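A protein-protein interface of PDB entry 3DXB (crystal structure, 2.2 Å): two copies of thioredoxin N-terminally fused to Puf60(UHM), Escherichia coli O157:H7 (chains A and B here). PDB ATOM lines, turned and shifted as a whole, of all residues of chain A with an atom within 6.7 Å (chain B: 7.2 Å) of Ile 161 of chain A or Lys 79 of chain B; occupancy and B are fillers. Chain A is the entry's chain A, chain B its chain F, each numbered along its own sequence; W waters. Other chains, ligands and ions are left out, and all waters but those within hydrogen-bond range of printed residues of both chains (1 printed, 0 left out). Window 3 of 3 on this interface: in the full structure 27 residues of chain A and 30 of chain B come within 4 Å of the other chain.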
ATOM      1  N   VAL A 133       2.316  19.288   0.148  1.00  0.00           N
ATOM      2  CA  VAL A 133       1.001  19.913   0.185  1.00  0.00           C
ATOM      3  C   VAL A 133       0.041  19.040   0.992  1.00  0.00           C
ATOM      4  O   VAL A 133      -0.025  17.826   0.784  1.00  0.00           O
ATOM      5  CB  VAL A 133       0.454  20.140  -1.260  1.00  0.00           C
ATOM      6  CG1 VAL A 133      -0.989  20.612  -1.242  1.00  0.00           C
ATOM      7  CG2 VAL A 133       1.319  21.144  -2.018  1.00  0.00           C
ATOM      8  N   ILE A 138      -4.750  22.028  -1.372  1.00  0.00           N
ATOM      9  CA  ILE A 138      -5.001  21.902  -2.808  1.00  0.00           C
ATOM     10  C   ILE A 138      -6.103  22.857  -3.264  1.00  0.00           C
ATOM     11  O   ILE A 138      -7.177  22.912  -2.662  1.00  0.00           O
ATOM     12  CB  ILE A 138      -5.401  20.455  -3.207  1.00  0.00           C
ATOM     13  CG1 ILE A 138      -4.364  19.440  -2.717  1.00  0.00           C
ATOM     14  CG2 ILE A 138      -5.598  20.340  -4.726  1.00  0.00           C
ATOM     15  CD1 ILE A 138      -4.820  17.997  -2.837  1.00  0.00           C
ATOM     16  N   ASP A 139      -5.818  23.621  -4.316  1.00  0.00           N
ATOM     17  CA  ASP A 139      -6.841  24.414  -4.994  1.00  0.00           C
ATOM     18  C   ASP A 139      -6.665  24.353  -6.512  1.00  0.00           C
ATOM     19  O   ASP A 139      -5.816  23.615  -7.013  1.00  0.00           O
ATOM     20  CB  ASP A 139      -6.869  25.862  -4.478  1.00  0.00           C
ATOM     21  CG  ASP A 139      -5.525  26.567  -4.597  1.00  0.00           C
ATOM     22  OD1 ASP A 139      -4.800  26.346  -5.590  1.00  0.00           O
ATOM     23  OD2 ASP A 139      -5.198  27.361  -3.689  1.00  0.00           O
ATOM     24  N   LEU A 142      -2.962  25.112  -7.941  1.00  0.00           N
ATOM     25  CA  LEU A 142      -1.794  24.306  -7.553  1.00  0.00           C
ATOM     26  C   LEU A 142      -1.089  23.581  -8.705  1.00  0.00           C
ATOM     27  O   LEU A 142       0.138  23.627  -8.806  1.00  0.00           O
ATOM     28  CB  LEU A 142      -2.159  23.315  -6.436  1.00  0.00           C
ATOM     29  CG  LEU A 142      -1.036  22.468  -5.820  1.00  0.00           C
ATOM     30  CD1 LEU A 142       0.002  23.328  -5.106  1.00  0.00           C
ATOM     31  CD2 LEU A 142      -1.606  21.426  -4.871  1.00  0.00           C
ATOM     32  N   GLU A 143      -1.864  22.908  -9.554  1.00  0.00           N
ATOM     33  CA  GLU A 143      -1.315  22.221 -10.721  1.00  0.00           C
ATOM     34  C   GLU A 143      -0.532  23.204 -11.590  1.00  0.00           C
ATOM     35  O   GLU A 143       0.616  22.942 -11.941  1.00  0.00           O
ATOM     36  CB  GLU A 143      -2.427  21.553 -11.535  1.00  0.00           C
ATOM     37  CG  GLU A 143      -1.933  20.774 -12.753  1.00  0.00           C
ATOM     38  CD  GLU A 143      -3.065  20.248 -13.621  1.00  0.00           C
ATOM     39  OE1 GLU A 143      -2.913  20.241 -14.860  1.00  0.00           O
ATOM     40  OE2 GLU A 143      -4.108  19.843 -13.069  1.00  0.00           O
ATOM     41  N   VAL A 146       2.751  24.434  -9.972  1.00  0.00           N
ATOM     42  CA  VAL A 146       3.773  23.385 -10.014  1.00  0.00           C
ATOM     43  C   VAL A 146       4.420  23.278 -11.400  1.00  0.00           C
ATOM     44  O   VAL A 146       5.648  23.263 -11.511  1.00  0.00           O
ATOM     45  CB  VAL A 146       3.211  22.007  -9.555  1.00  0.00           C
ATOM     46  CG1 VAL A 146       4.219  20.893  -9.808  1.00  0.00           C
ATOM     47  CG2 VAL A 146       2.840  22.047  -8.079  1.00  0.00           C
ATOM     48  N   ARG A 158       3.050  16.795 -18.007  1.00  0.00           N
ATOM     49  CA  ARG A 158       1.828  16.687 -17.229  1.00  0.00           C
ATOM     50  C   ARG A 158       2.178  16.800 -15.755  1.00  0.00           C
ATOM     51  O   ARG A 158       3.258  16.375 -15.329  1.00  0.00           O
ATOM     52  CB  ARG A 158       1.127  15.344 -17.500  1.00  0.00           C
ATOM     53  CG  ARG A 158      -0.383  15.358 -17.237  1.00  0.00           C
ATOM     54  CD  ARG A 158      -0.984  13.951 -17.231  1.00  0.00           C
ATOM     55  NE  ARG A 158      -2.452  13.958 -17.220  1.00  0.00           N
ATOM     56  CZ  ARG A 158      -3.223  12.867 -17.228  1.00  0.00           C
ATOM     57  NH1 ARG A 158      -2.680  11.656 -17.244  1.00  0.00           N
ATOM     58  NH2 ARG A 158      -4.544  12.982 -17.221  1.00  0.00           N
ATOM     59  N   VAL A 159       1.268  17.394 -14.990  1.00  0.00           N
ATOM     60  CA  VAL A 159       1.378  17.443 -13.536  1.00  0.00           C
ATOM     61  C   VAL A 159       0.134  16.796 -12.942  1.00  0.00           C
ATOM     62  O   VAL A 159      -0.988  17.132 -13.323  1.00  0.00           O
ATOM     63  CB  VAL A 159       1.548  18.893 -13.006  1.00  0.00           C
ATOM     64  CG1 VAL A 159       1.290  18.967 -11.500  1.00  0.00           C
ATOM     65  CG2 VAL A 159       2.938  19.414 -13.322  1.00  0.00           C
ATOM     66  N   ILE A 160       0.338  15.858 -12.021  1.00  0.00           N
ATOM     67  CA  ILE A 160      -0.780  15.195 -11.355  1.00  0.00           C
ATOM     68  C   ILE A 160      -0.772  15.441  -9.847  1.00  0.00           C
ATOM     69  O   ILE A 160       0.217  15.161  -9.164  1.00  0.00           O
ATOM     70  CB  ILE A 160      -0.833  13.682 -11.691  1.00  0.00           C
ATOM     71  CG1 ILE A 160      -1.092  13.497 -13.192  1.00  0.00           C
ATOM     72  CG2 ILE A 160      -1.918  12.971 -10.855  1.00  0.00           C
ATOM     73  CD1 ILE A 160      -0.888  12.097 -13.699  1.00  0.00           C
ATOM     74  N   ILE A 161      -1.874  16.001  -9.351  1.00  0.00           N
ATOM     75  CA  ILE A 161      -2.101  16.151  -7.918  1.00  0.00           C
ATOM     76  C   ILE A 161      -2.892  14.929  -7.449  1.00  0.00           C
ATOM     77  O   ILE A 161      -4.080  14.787  -7.753  1.00  0.00           O
ATOM     78  CB  ILE A 161      -2.844  17.480  -7.576  1.00  0.00           C
ATOM     79  CG1 ILE A 161      -2.175  18.692  -8.254  1.00  0.00           C
ATOM     80  CG2 ILE A 161      -2.967  17.670  -6.059  1.00  0.00           C
ATOM     81  CD1 ILE A 161      -0.739  18.988  -7.819  1.00  0.00           C
ATOM     82  N   TYR A 162      -2.210  14.044  -6.728  1.00  0.00           N
ATOM     83  CA  TYR A 162      -2.765  12.752  -6.352  1.00  0.00           C
ATOM     84  C   TYR A 162      -2.966  12.648  -4.847  1.00  0.00           C
ATOM     85  O   TYR A 162      -2.046  12.879  -4.065  1.00  0.00           O
ATOM     86  CB  TYR A 162      -1.852  11.627  -6.844  1.00  0.00           C
ATOM     87  CG  TYR A 162      -2.384  10.224  -6.641  1.00  0.00           C
ATOM     88  CD1 TYR A 162      -3.458   9.746  -7.396  1.00  0.00           C
ATOM     89  CD2 TYR A 162      -1.794   9.361  -5.715  1.00  0.00           C
ATOM     90  CE1 TYR A 162      -3.942   8.455  -7.225  1.00  0.00           C
ATOM     91  CE2 TYR A 162      -2.270   8.061  -5.539  1.00  0.00           C
ATOM     92  CZ  TYR A 162      -3.345   7.618  -6.297  1.00  0.00           C
ATOM     93  OH  TYR A 162      -3.825   6.337  -6.133  1.00  0.00           O
ATOM     94  N   GLN A 163      -4.183  12.296  -4.456  1.00  0.00           N
ATOM     95  CA  GLN A 163      -4.511  12.115  -3.049  1.00  0.00           C
ATOM     96  C   GLN A 163      -4.624  10.627  -2.745  1.00  0.00           C
ATOM     97  O   GLN A 163      -5.311   9.892  -3.458  1.00  0.00           O
ATOM     98  CB  GLN A 163      -5.803  12.851  -2.708  1.00  0.00           C
ATOM     99  CG  GLN A 163      -5.749  14.347  -2.991  1.00  0.00           C
ATOM    100  CD  GLN A 163      -7.014  15.061  -2.570  1.00  0.00           C
ATOM    101  OE1 GLN A 163      -7.385  15.047  -1.398  1.00  0.00           O
ATOM    102  NE2 GLN A 163      -7.684  15.690  -3.526  1.00  0.00           N
ATOM    103  N   VAL A 176      -0.821  13.764  -0.065  1.00  0.00           N
ATOM    104  CA  VAL A 176      -0.724  14.226  -1.445  1.00  0.00           C
ATOM    105  C   VAL A 176       0.632  13.857  -2.045  1.00  0.00           C
ATOM    106  O   VAL A 176       1.685  14.115  -1.450  1.00  0.00           O
ATOM    107  CB  VAL A 176      -0.969  15.758  -1.560  1.00  0.00           C
ATOM    108  CG1 VAL A 176      -0.960  16.215  -3.019  1.00  0.00           C
ATOM    109  CG2 VAL A 176      -2.290  16.139  -0.898  1.00  0.00           C
ATOM    110  N   LYS A 177       0.591  13.224  -3.212  1.00  0.00           N
ATOM    111  CA  LYS A 177       1.782  13.019  -4.023  1.00  0.00           C
ATOM    112  C   LYS A 177       1.625  13.877  -5.261  1.00  0.00           C
ATOM    113  O   LYS A 177       0.598  13.799  -5.944  1.00  0.00           O
ATOM    114  CB  LYS A 177       1.923  11.563  -4.472  1.00  0.00           C
ATOM    115  CG  LYS A 177       1.802  10.497  -3.401  1.00  0.00           C
ATOM    116  CD  LYS A 177       1.622   9.155  -4.092  1.00  0.00           C
ATOM    117  CE  LYS A 177       1.873   7.994  -3.168  1.00  0.00           C
ATOM    118  NZ  LYS A 177       1.798   6.715  -3.923  1.00  0.00           N
ATOM    119  N   ILE A 178       2.633  14.693  -5.551  1.00  0.00           N
ATOM    120  CA  ILE A 178       2.624  15.513  -6.758  1.00  0.00           C
ATOM    121  C   ILE A 178       3.561  14.927  -7.807  1.00  0.00           C
ATOM    122  O   ILE A 178       4.782  14.881  -7.616  1.00  0.00           O
ATOM    123  CB  ILE A 178       2.985  16.989  -6.474  1.00  0.00           C
ATOM    124  CG1 ILE A 178       1.987  17.595  -5.481  1.00  0.00           C
ATOM    125  CG2 ILE A 178       2.996  17.789  -7.777  1.00  0.00           C
ATOM    126  CD1 ILE A 178       2.399  18.947  -4.924  1.00  0.00           C
ATOM    127  N   PHE A 179       2.971  14.480  -8.911  1.00  0.00           N
ATOM    128  CA  PHE A 179       3.724  13.891 -10.010  1.00  0.00           C
ATOM    129  C   PHE A 179       4.023  14.942 -11.067  1.00  0.00           C
ATOM    130  O   PHE A 179       3.134  15.678 -11.497  1.00  0.00           O
ATOM    131  CB  PHE A 179       2.952  12.724 -10.638  1.00  0.00           C
ATOM    132  CG  PHE A 179       2.752  11.556  -9.710  1.00  0.00           C
ATOM    133  CD1 PHE A 179       3.688  10.526  -9.657  1.00  0.00           C
ATOM    134  CD2 PHE A 179       1.626  11.483  -8.894  1.00  0.00           C
ATOM    135  CE1 PHE A 179       3.509   9.444  -8.799  1.00  0.00           C
ATOM    136  CE2 PHE A 179       1.435  10.406  -8.033  1.00  0.00           C
ATOM    137  CZ  PHE A 179       2.379   9.382  -7.983  1.00  0.00           C
ATOM    138  N   LEU A 220      -0.357   4.984  -9.536  1.00  0.00           N
ATOM    139  CA  LEU A 220       0.262   6.086  -8.798  1.00  0.00           C
ATOM    140  C   LEU A 220       0.463   5.734  -7.323  1.00  0.00           C
ATOM    141  O   LEU A 220       0.658   6.616  -6.480  1.00  0.00           O
ATOM    142  CB  LEU A 220      -0.570   7.369  -8.955  1.00  0.00           C
ATOM    143  CG  LEU A 220      -0.945   7.824 -10.375  1.00  0.00           C
ATOM    144  CD1 LEU A 220      -1.690   9.141 -10.328  1.00  0.00           C
ATOM    145  CD2 LEU A 220       0.272   7.947 -11.286  1.00  0.00           C
ATOM    146  N   ASP B  19     -18.838  13.323 -11.659  1.00  0.00           N
ATOM    147  CA  ASP B  19     -17.756  13.979 -10.919  1.00  0.00           C
ATOM    148  C   ASP B  19     -18.175  14.321  -9.490  1.00  0.00           C
ATOM    149  O   ASP B  19     -17.364  14.258  -8.567  1.00  0.00           O
ATOM    150  CB  ASP B  19     -17.278  15.244 -11.643  1.00  0.00           C
ATOM    151  CG  ASP B  19     -16.372  14.941 -12.825  1.00  0.00           C
ATOM    152  OD1 ASP B  19     -16.258  15.810 -13.715  1.00  0.00           O
ATOM    153  OD2 ASP B  19     -15.772  13.844 -12.872  1.00  0.00           O
ATOM    154  N   PRO B  74     -15.332  15.291 -16.864  1.00  0.00           N
ATOM    155  CA  PRO B  74     -13.898  15.403 -17.145  1.00  0.00           C
ATOM    156  C   PRO B  74     -13.009  15.697 -15.931  1.00  0.00           C
ATOM    157  O   PRO B  74     -11.787  15.752 -16.071  1.00  0.00           O
ATOM    158  CB  PRO B  74     -13.836  16.567 -18.136  1.00  0.00           C
ATOM    159  CG  PRO B  74     -14.997  17.439 -17.762  1.00  0.00           C
ATOM    160  CD  PRO B  74     -16.039  16.566 -17.097  1.00  0.00           C
ATOM    161  N   GLY B  75     -13.610  15.874 -14.757  1.00  0.00           N
ATOM    162  CA  GLY B  75     -12.860  16.260 -13.565  1.00  0.00           C
ATOM    163  C   GLY B  75     -12.109  15.144 -12.861  1.00  0.00           C
ATOM    164  O   GLY B  75     -11.007  15.358 -12.349  1.00  0.00           O
ATOM    165  N   THR B  76     -12.703  13.953 -12.836  1.00  0.00           N
ATOM    166  CA  THR B  76     -12.199  12.847 -12.022  1.00  0.00           C
ATOM    167  C   THR B  76     -10.957  12.152 -12.595  1.00  0.00           C
ATOM    168  O   THR B  76      -9.971  11.973 -11.880  1.00  0.00           O
ATOM    169  CB  THR B  76     -13.311  11.800 -11.733  1.00  0.00           C
ATOM    170  OG1 THR B  76     -14.437  12.446 -11.127  1.00  0.00           O
ATOM    171  CG2 THR B  76     -12.807  10.700 -10.807  1.00  0.00           C
ATOM    172  N   ALA B  77     -11.007  11.768 -13.870  1.00  0.00           N
ATOM    173  CA  ALA B  77      -9.964  10.924 -14.475  1.00  0.00           C
ATOM    174  C   ALA B  77      -8.524  11.467 -14.409  1.00  0.00           C
ATOM    175  O   ALA B  77      -7.610  10.708 -14.077  1.00  0.00           O
ATOM    176  CB  ALA B  77     -10.344  10.516 -15.903  1.00  0.00           C
ATOM    177  N   PRO B  78      -8.306  12.768 -14.719  1.00  0.00           N
ATOM    178  CA  PRO B  78      -6.947  13.321 -14.577  1.00  0.00           C
ATOM    179  C   PRO B  78      -6.377  13.256 -13.156  1.00  0.00           C
ATOM    180  O   PRO B  78      -5.158  13.305 -12.983  1.00  0.00           O
ATOM    181  CB  PRO B  78      -7.114  14.784 -15.008  1.00  0.00           C
ATOM    182  CG  PRO B  78      -8.316  14.783 -15.874  1.00  0.00           C
ATOM    183  CD  PRO B  78      -9.237  13.784 -15.247  1.00  0.00           C
ATOM    184  N   LYS B  79      -7.249  13.138 -12.157  1.00  0.00           N
ATOM    185  CA  LYS B  79      -6.821  13.030 -10.758  1.00  0.00           C
ATOM    186  C   LYS B  79      -6.227  11.655 -10.445  1.00  0.00           C
ATOM    187  O   LYS B  79      -5.529  11.483  -9.446  1.00  0.00           O
ATOM    188  CB  LYS B  79      -7.982  13.334  -9.811  1.00  0.00           C
ATOM    189  CG  LYS B  79      -8.544  14.739  -9.953  1.00  0.00           C
ATOM    190  CD  LYS B  79      -9.728  14.954  -9.028  1.00  0.00           C
ATOM    191  CE  LYS B  79     -10.308  16.346  -9.202  1.00  0.00           C
ATOM    192  NZ  LYS B  79     -11.548  16.517  -8.396  1.00  0.00           N
ATOM    193  N   TYR B  80      -6.507  10.683 -11.311  1.00  0.00           N
ATOM    194  CA  TYR B  80      -6.000   9.324 -11.146  1.00  0.00           C
ATOM    195  C   TYR B  80      -4.956   8.958 -12.205  1.00  0.00           C
ATOM    196  O   TYR B  80      -4.510   7.810 -12.286  1.00  0.00           O
ATOM    197  CB  TYR B  80      -7.160   8.326 -11.119  1.00  0.00           C
ATOM    198  CG  TYR B  80      -7.965   8.404  -9.840  1.00  0.00           C
ATOM    199  CD1 TYR B  80      -9.154   9.131  -9.781  1.00  0.00           C
ATOM    200  CD2 TYR B  80      -7.523   7.768  -8.679  1.00  0.00           C
ATOM    201  CE1 TYR B  80      -9.890   9.208  -8.599  1.00  0.00           C
ATOM    202  CE2 TYR B  80      -8.245   7.840  -7.498  1.00  0.00           C
ATOM    203  CZ  TYR B  80      -9.424   8.561  -7.464  1.00  0.00           C
ATOM    204  OH  TYR B  80     -10.139   8.626  -6.297  1.00  0.00           O
ATOM    205  N   GLY B  81      -4.557   9.953 -12.995  1.00  0.00           N
ATOM    206  CA  GLY B  81      -3.549   9.772 -14.031  1.00  0.00           C
ATOM    207  C   GLY B  81      -4.036   8.935 -15.196  1.00  0.00           C
ATOM    208  O   GLY B  81      -3.262   8.184 -15.797  1.00  0.00           O
ATOM    209  N   ILE B  82      -5.322   9.057 -15.511  1.00  0.00           N
ATOM    210  CA  ILE B  82      -5.906   8.325 -16.630  1.00  0.00           C
ATOM    211  C   ILE B  82      -5.455   8.952 -17.945  1.00  0.00           C
ATOM    212  O   ILE B  82      -5.493  10.172 -18.108  1.00  0.00           O
ATOM    213  CB  ILE B  82      -7.460   8.255 -16.543  1.00  0.00           C
ATOM    214  CG1 ILE B  82      -7.919   7.675 -15.192  1.00  0.00           C
ATOM    215  CG2 ILE B  82      -8.050   7.468 -17.720  1.00  0.00           C
ATOM    216  CD1 ILE B  82      -7.394   6.275 -14.871  1.00  0.00           C
HETATM  217  O   HOH W   1      -6.430  11.653  -6.821  1.00  0.00           O
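Arg 158 of chain A touches Pro 78 of chain B.
Gly 81 of chain B touches Arg 158 of chain A (C to NH1, 3.7 Å).
O of Pro 78 of chain B touches CG2 of Ile 160 of chain A, at 3.9 Å.
CD1 of Ile 160 of chain A touches CA of Gly 81 of chain B, 3.5 Å away.
Ile 161 of chain A touches Lys 79 of chain B.
Lys 79 of chain B touches Tyr 162 of chain A (O to CD1, 3.4 Å).
Tyr 80 of chain B touches Tyr 162 of chain A.
Leu 220 of chain A touches Tyr 80 of chain B.
Leu 220 of chain A touches Gly 81 of chain B (CD1 to N, 3.999 Å).
Hydrophobic or aromatic side chains of chain A within 4 Å of the printed part of chain B: Ile 160, Tyr 162 and Leu 220.
Of the 10 printed residues of chain B, 5 touch a printed residue of chain A.
Among the printed residues, 10 pairs touch across the chains.
No position is printed for both chains.
Of the 10 pairs that touch across the chains among the printed residues, none has its exchanged pair printed and touching as well.
Water W1 lies within hydrogen-bond range of O of Lys 79 of chain B (2.8 Å) and N of Gln 163 of chain A (3.3 Å).
The backbone carbonyl oxygen (O) of Ile 160 of chain A is in hydrogen-bond range of the backbone NH (N) of Phe 179 of chain A, 2.8 Å away.
The backbone carbonyl oxygen (O) of Tyr 162 of chain A is in hydrogen-bond range of the backbone NH (N) of Lys 177 of chain A, at 2.8 Å.
The side-chain amino group (NZ) of Lys 177 of chain A lies within hydrogen-bond range of the backbone carbonyl oxygen (O) of Leu 220 of chain A (2.8 Å).
N of Ile 82 of chain B sits at hydrogen-bond distance from O of Ala 77 of chain B, at 3.2 Å.
The backbone carbonyl oxygen (O) of Ile 82 of chain B is in hydrogen-bond range of the guanidinium group (NH2) of Arg 158 of chain A, 3.1 Å away.
Of the printed residues of chain B, Ile 161 of chain A touches Lys 79.
Printed residues of chain B within 4 Å of Tyr 162 of chain A: Lys 79 (3.4 Å) and Tyr 80 (3.9 Å).
Gln 163 of chain A touches none of the printed residues of chain B.
Of the printed residues of chain B, Leu 220 of chain A touches Tyr 80 (3.7 Å) and Gly 81 (3.999 Å).
Of the printed residues of chain A, Lys 79 of chain B touches Ile 161 (3.99 Å) and Tyr 162 (3.4 Å).
Of the printed residues of chain A, Tyr 80 of chain B touches Tyr 162 (3.9 Å) and Leu 220 (3.7 Å).
Printed residues of chain A within 4 Å of Gly 81 of chain B: Arg 158, Ile 160 and Leu 220.
Printed residues of chain A within 4 Å of Ile 82 of chain B: Arg 158 (3.1 Å).
The nearest printed residue of chain B that does not touch Ile 161 of chain A is Pro 78 of chain B (5.5 Å).
The nearest printed residue of chain A that does not touch Lys 79 of chain B is Ile 160 of chain A (4.2 Å).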
